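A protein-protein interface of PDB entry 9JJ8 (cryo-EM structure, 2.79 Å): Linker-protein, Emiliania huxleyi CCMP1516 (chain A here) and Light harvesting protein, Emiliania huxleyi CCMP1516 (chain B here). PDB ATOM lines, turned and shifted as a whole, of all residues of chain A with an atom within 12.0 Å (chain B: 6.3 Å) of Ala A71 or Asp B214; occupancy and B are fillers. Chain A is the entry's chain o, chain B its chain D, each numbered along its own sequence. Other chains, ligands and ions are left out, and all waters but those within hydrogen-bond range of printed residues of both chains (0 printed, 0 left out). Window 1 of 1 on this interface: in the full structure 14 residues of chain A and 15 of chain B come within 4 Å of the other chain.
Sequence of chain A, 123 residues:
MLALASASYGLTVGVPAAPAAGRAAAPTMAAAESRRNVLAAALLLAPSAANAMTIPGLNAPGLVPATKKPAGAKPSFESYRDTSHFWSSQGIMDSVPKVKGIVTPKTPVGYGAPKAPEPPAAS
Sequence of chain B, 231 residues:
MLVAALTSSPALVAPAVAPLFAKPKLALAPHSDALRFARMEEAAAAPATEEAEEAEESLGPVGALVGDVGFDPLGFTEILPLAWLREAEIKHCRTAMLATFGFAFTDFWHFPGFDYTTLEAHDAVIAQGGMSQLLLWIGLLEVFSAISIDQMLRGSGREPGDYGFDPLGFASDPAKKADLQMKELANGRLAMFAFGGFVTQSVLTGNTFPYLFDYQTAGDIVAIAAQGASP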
ATOM      1  N   THR A  67     -41.027 -21.043  13.707  1.00  0.00           N
ATOM      2  CA  THR A  67     -40.090 -21.025  12.592  1.00  0.00           C
ATOM      3  C   THR A  67     -38.652 -21.003  13.113  1.00  0.00           C
ATOM      4  O   THR A  67     -38.305 -20.209  13.995  1.00  0.00           O
ATOM      5  CB  THR A  67     -40.389 -19.845  11.659  1.00  0.00           C
ATOM      6  OG1 THR A  67     -39.472 -19.845  10.557  1.00  0.00           O
ATOM      7  CG2 THR A  67     -40.380 -18.490  12.383  1.00  0.00           C
ATOM      8  N   LYS A  68     -37.836 -21.922  12.610  1.00  0.00           N
ATOM      9  CA  LYS A  68     -36.472 -22.066  13.090  1.00  0.00           C
ATOM     10  C   LYS A  68     -35.557 -21.057  12.413  1.00  0.00           C
ATOM     11  O   LYS A  68     -35.728 -20.717  11.238  1.00  0.00           O
ATOM     12  CB  LYS A  68     -35.962 -23.487  12.847  1.00  0.00           C
ATOM     13  CG  LYS A  68     -36.694 -24.558  13.647  1.00  0.00           C
ATOM     14  CD  LYS A  68     -36.558 -24.319  15.144  1.00  0.00           C
ATOM     15  CE  LYS A  68     -37.117 -25.484  15.949  1.00  0.00           C
ATOM     16  NZ  LYS A  68     -38.576 -25.677  15.720  1.00  0.00           N
ATOM     17  N   LYS A  69     -34.575 -20.574  13.171  1.00  0.00           N
ATOM     18  CA  LYS A  69     -33.659 -19.562  12.682  1.00  0.00           C
ATOM     19  C   LYS A  69     -32.220 -19.991  12.933  1.00  0.00           C
ATOM     20  O   LYS A  69     -31.893 -20.462  14.029  1.00  0.00           O
ATOM     21  CB  LYS A  69     -33.927 -18.212  13.364  1.00  0.00           C
ATOM     22  CG  LYS A  69     -33.310 -17.021  12.657  1.00  0.00           C
ATOM     23  CD  LYS A  69     -33.629 -15.730  13.385  1.00  0.00           C
ATOM     24  CE  LYS A  69     -32.890 -15.657  14.706  1.00  0.00           C
ATOM     25  NZ  LYS A  69     -31.432 -15.418  14.516  1.00  0.00           N
ATOM     26  N   PRO A  70     -31.346 -19.855  11.938  1.00  0.00           N
ATOM     27  CA  PRO A  70     -29.925 -20.148  12.157  1.00  0.00           C
ATOM     28  C   PRO A  70     -29.278 -19.120  13.072  1.00  0.00           C
ATOM     29  O   PRO A  70     -29.748 -17.990  13.223  1.00  0.00           O
ATOM     30  CB  PRO A  70     -29.327 -20.094  10.747  1.00  0.00           C
ATOM     31  CG  PRO A  70     -30.272 -19.239   9.968  1.00  0.00           C
ATOM     32  CD  PRO A  70     -31.632 -19.521  10.533  1.00  0.00           C
ATOM     33  N   ALA A  71     -28.177 -19.536  13.693  1.00  0.00           N
ATOM     34  CA  ALA A  71     -27.484 -18.732  14.691  1.00  0.00           C
ATOM     35  C   ALA A  71     -26.330 -17.974  14.049  1.00  0.00           C
ATOM     36  O   ALA A  71     -25.575 -18.542  13.251  1.00  0.00           O
ATOM     37  CB  ALA A  71     -26.964 -19.612  15.828  1.00  0.00           C
ATOM     38  N   GLY A  72     -26.193 -16.694  14.396  1.00  0.00           N
ATOM     39  CA  GLY A  72     -25.088 -15.910  13.883  1.00  0.00           C
ATOM     40  C   GLY A  72     -25.076 -14.445  14.264  1.00  0.00           C
ATOM     41  O   GLY A  72     -26.140 -13.850  14.466  1.00  0.00           O
ATOM     42  N   ALA A  73     -23.871 -13.866  14.378  1.00  0.00           N
ATOM     43  CA  ALA A  73     -23.673 -12.418  14.301  1.00  0.00           C
ATOM     44  C   ALA A  73     -24.389 -11.600  15.372  1.00  0.00           C
ATOM     45  O   ALA A  73     -25.486 -11.095  15.107  1.00  0.00           O
ATOM     46  CB  ALA A  73     -24.087 -11.909  12.916  1.00  0.00           C
ATOM     47  N   LYS A  74     -23.850 -11.579  16.612  1.00  0.00           N
ATOM     48  CA  LYS A  74     -24.256 -10.619  17.643  1.00  0.00           C
ATOM     49  C   LYS A  74     -24.380  -9.235  17.015  1.00  0.00           C
ATOM     50  O   LYS A  74     -23.373  -8.656  16.583  1.00  0.00           O
ATOM     51  CB  LYS A  74     -23.246 -10.582  18.794  1.00  0.00           C
ATOM     52  CG  LYS A  74     -23.410  -9.377  19.722  1.00  0.00           C
ATOM     53  CD  LYS A  74     -22.353  -9.326  20.815  1.00  0.00           C
ATOM     54  CE  LYS A  74     -22.563  -8.107  21.704  1.00  0.00           C
ATOM     55  NZ  LYS A  74     -21.696  -8.126  22.914  1.00  0.00           N
ATOM     56  N   PRO A  75     -25.612  -8.697  16.912  1.00  0.00           N
ATOM     57  CA  PRO A  75     -25.888  -7.642  15.921  1.00  0.00           C
ATOM     58  C   PRO A  75     -25.155  -6.331  16.146  1.00  0.00           C
ATOM     59  O   PRO A  75     -24.321  -5.935  15.324  1.00  0.00           O
ATOM     60  CB  PRO A  75     -27.407  -7.438  16.049  1.00  0.00           C
ATOM     61  CG  PRO A  75     -27.914  -8.624  16.830  1.00  0.00           C
ATOM     62  CD  PRO A  75     -26.795  -9.016  17.726  1.00  0.00           C
ATOM     63  N   SER A  76     -25.428  -5.694  17.285  1.00  0.00           N
ATOM     64  CA  SER A  76     -24.825  -4.458  17.772  1.00  0.00           C
ATOM     65  C   SER A  76     -25.489  -4.141  19.101  1.00  0.00           C
ATOM     66  O   SER A  76     -26.607  -4.587  19.365  1.00  0.00           O
ATOM     67  CB  SER A  76     -25.013  -3.278  16.807  1.00  0.00           C
ATOM     68  OG  SER A  76     -24.261  -2.154  17.223  1.00  0.00           O
ATOM     69  N   GLY B 206     -29.346 -13.085  19.762  1.00  0.00           N
ATOM     70  CA  GLY B 206     -30.388 -13.113  18.756  1.00  0.00           C
ATOM     71  C   GLY B 206     -30.623 -14.500  18.200  1.00  0.00           C
ATOM     72  O   GLY B 206     -30.767 -14.668  16.986  1.00  0.00           O
ATOM     73  N   ASN B 207     -30.659 -15.504  19.073  1.00  0.00           N
ATOM     74  CA  ASN B 207     -30.844 -16.890  18.670  1.00  0.00           C
ATOM     75  C   ASN B 207     -31.904 -17.543  19.552  1.00  0.00           C
ATOM     76  O   ASN B 207     -32.393 -16.952  20.520  1.00  0.00           O
ATOM     77  CB  ASN B 207     -29.525 -17.671  18.738  1.00  0.00           C
ATOM     78  CG  ASN B 207     -28.386 -16.954  18.042  1.00  0.00           C
ATOM     79  OD1 ASN B 207     -28.510 -16.543  16.890  1.00  0.00           O
ATOM     80  ND2 ASN B 207     -27.266 -16.807  18.736  1.00  0.00           N
ATOM     81  N   LEU B 212     -26.834 -18.887  22.403  1.00  0.00           N
ATOM     82  CA  LEU B 212     -25.382 -18.884  22.323  1.00  0.00           C
ATOM     83  C   LEU B 212     -24.945 -18.174  21.051  1.00  0.00           C
ATOM     84  O   LEU B 212     -25.712 -18.033  20.096  1.00  0.00           O
ATOM     85  CB  LEU B 212     -24.810 -20.309  22.348  1.00  0.00           C
ATOM     86  CG  LEU B 212     -25.193 -21.183  23.542  1.00  0.00           C
ATOM     87  CD1 LEU B 212     -24.899 -22.649  23.264  1.00  0.00           C
ATOM     88  CD2 LEU B 212     -24.468 -20.718  24.790  1.00  0.00           C
ATOM     89  N   PHE B 213     -23.694 -17.723  21.055  1.00  0.00           N
ATOM     90  CA  PHE B 213     -23.126 -17.077  19.884  1.00  0.00           C
ATOM     91  C   PHE B 213     -22.870 -18.103  18.782  1.00  0.00           C
ATOM     92  O   PHE B 213     -22.954 -19.317  18.991  1.00  0.00           O
ATOM     93  CB  PHE B 213     -21.825 -16.361  20.246  1.00  0.00           C
ATOM     94  CG  PHE B 213     -22.015 -15.163  21.135  1.00  0.00           C
ATOM     95  CD1 PHE B 213     -22.544 -13.985  20.636  1.00  0.00           C
ATOM     96  CD2 PHE B 213     -21.647 -15.212  22.471  1.00  0.00           C
ATOM     97  CE1 PHE B 213     -22.713 -12.883  21.454  1.00  0.00           C
ATOM     98  CE2 PHE B 213     -21.812 -14.110  23.292  1.00  0.00           C
ATOM     99  CZ  PHE B 213     -22.347 -12.946  22.782  1.00  0.00           C
ATOM    100  N   ASP B 214     -22.557 -17.596  17.587  1.00  0.00           N
ATOM    101  CA  ASP B 214     -22.317 -18.478  16.448  1.00  0.00           C
ATOM    102  C   ASP B 214     -21.042 -19.292  16.610  1.00  0.00           C
ATOM    103  O   ASP B 214     -20.984 -20.441  16.158  1.00  0.00           O
ATOM    104  CB  ASP B 214     -22.260 -17.667  15.156  1.00  0.00           C
ATOM    105  CG  ASP B 214     -21.292 -16.507  15.235  1.00  0.00           C
ATOM    106  OD1 ASP B 214     -21.089 -15.977  16.347  1.00  0.00           O
ATOM    107  OD2 ASP B 214     -20.742 -16.118  14.184  1.00  0.00           O
ATOM    108  N   TYR B 215     -20.017 -18.730  17.249  1.00  0.00           N
ATOM    109  CA  TYR B 215     -18.772 -19.462  17.427  1.00  0.00           C
ATOM    110  C   TYR B 215     -18.846 -20.498  18.540  1.00  0.00           C
ATOM    111  O   TYR B 215     -17.939 -21.330  18.648  1.00  0.00           O
ATOM    112  CB  TYR B 215     -17.617 -18.488  17.688  1.00  0.00           C
ATOM    113  CG  TYR B 215     -17.851 -17.476  18.792  1.00  0.00           C
ATOM    114  CD1 TYR B 215     -17.619 -17.799  20.123  1.00  0.00           C
ATOM    115  CD2 TYR B 215     -18.282 -16.189  18.498  1.00  0.00           C
ATOM    116  CE1 TYR B 215     -17.823 -16.877  21.130  1.00  0.00           C
ATOM    117  CE2 TYR B 215     -18.487 -15.258  19.500  1.00  0.00           C
ATOM    118  CZ  TYR B 215     -18.257 -15.609  20.812  1.00  0.00           C
ATOM    119  OH  TYR B 215     -18.460 -14.688  21.813  1.00  0.00           O
ATOM    120  N   GLN B 216     -19.895 -20.475  19.362  1.00  0.00           N
ATOM    121  CA  GLN B 216     -20.068 -21.458  20.421  1.00  0.00           C
ATOM    122  C   GLN B 216     -20.870 -22.676  19.981  1.00  0.00           C
ATOM    123  O   GLN B 216     -20.903 -23.671  20.710  1.00  0.00           O
ATOM    124  CB  GLN B 216     -20.747 -20.811  21.635  1.00  0.00           C
ATOM    125  CG  GLN B 216     -19.919 -19.720  22.296  1.00  0.00           C
ATOM    126  CD  GLN B 216     -20.661 -19.021  23.416  1.00  0.00           C
ATOM    127  OE1 GLN B 216     -21.891 -18.996  23.441  1.00  0.00           O
ATOM    128  NE2 GLN B 216     -19.915 -18.443  24.350  1.00  0.00           N
ATOM    129  N   THR B 217     -21.514 -22.623  18.813  1.00  0.00           N
ATOM    130  CA  THR B 217     -22.265 -23.752  18.284  1.00  0.00           C
ATOM    131  C   THR B 217     -21.801 -24.209  16.910  1.00  0.00           C
ATOM    132  O   THR B 217     -21.919 -25.401  16.607  1.00  0.00           O
ATOM    133  CB  THR B 217     -23.763 -23.419  18.201  1.00  0.00           C
ATOM    134  OG1 THR B 217     -23.945 -22.199  17.472  1.00  0.00           O
ATOM    135  CG2 THR B 217     -24.357 -23.270  19.593  1.00  0.00           C
ATOM    136  N   ALA B 218     -21.282 -23.308  16.076  1.00  0.00           N
ATOM    137  CA  ALA B 218     -20.790 -23.648  14.747  1.00  0.00           C
ATOM    138  C   ALA B 218     -19.267 -23.693  14.701  1.00  0.00           C
ATOM    139  O   ALA B 218     -18.669 -23.660  13.625  1.00  0.00           O
ATOM    140  CB  ALA B 218     -21.326 -22.665  13.708  1.00  0.00           C
ATOM    141  N   GLY B 219     -18.629 -23.762  15.866  1.00  0.00           N
ATOM    142  CA  GLY B 219     -17.185 -23.846  15.931  1.00  0.00           C
ATOM    143  C   GLY B 219     -16.715 -24.959  16.841  1.00  0.00           C
ATOM    144  O   GLY B 219     -17.270 -26.062  16.823  1.00  0.00           O
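ND2 of Asn B207 lies within hydrogen-bond range of O of Leu B212 (2.4 Å).
The backbone NH (N) of Phe B213 is in hydrogen-bond range of the side-chain amide oxygen (OE1) of Gln B216.
The backbone carbonyl oxygen (O) of Phe B213 lies within hydrogen-bond range of the side-chain hydroxyl (OG1) of Thr B217, at 3.4 Å.
Printed residues of chain B within 4 Å of Lys A69: Gly B206 and Asn B207.
Of chain B, only Asn B207 (3.3 Å) and Asp B214 (3.9 Å) come within 4 Å of Ala A71.
Printed residues of chain B within 4 Å of Lys A74: Phe B213 (3.6 Å).
Of the printed residues of chain A, Phe B213 touches Lys A74.
Of chain A, only Ala A71, Gly A72 and Ala A73 come within 4 Å of Asp B214.
No residue of chain A comes within 4 Å of Tyr B215.
No residue of chain A comes within 4 Å of Gln B216.
Thr B217 touches none of the printed residues of chain A.
No residue of chain A comes within 4 Å of Ala B218.
Asn B207 touches Lys A69 (OD1 to NZ, 3.9 Å).
CA of Ala A71 touches OD1 of Asn B207, at 3.3 Å.
O of Ala A71 touches CB of Asp B214, at 3.9 Å.
CA of Gly A72 touches CB of Asp B214 (3.6 Å).
Asp B214 touches Ala A73 (CG to N, 3.8 Å).
Phe B213 touches Lys A74 (CE1 to CB, 3.6 Å).
The side-chain amino group of Lys A69 is in hydrogen-bond range of the backbone carbonyl oxygen of Gly B206, 2.7 Å away.
OD1 of Asn B207 is in hydrogen-bond range of N of Gly A72, at 3.4 Å.
Hydrophobic or aromatic side chains of chain B within 4 Å of the printed part of chain A: Phe B213.
Printed residues of chain A that touch a printed residue of chain B: Lys A69, Ala A71, Gly A72, Ala A73 and Lys A74.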
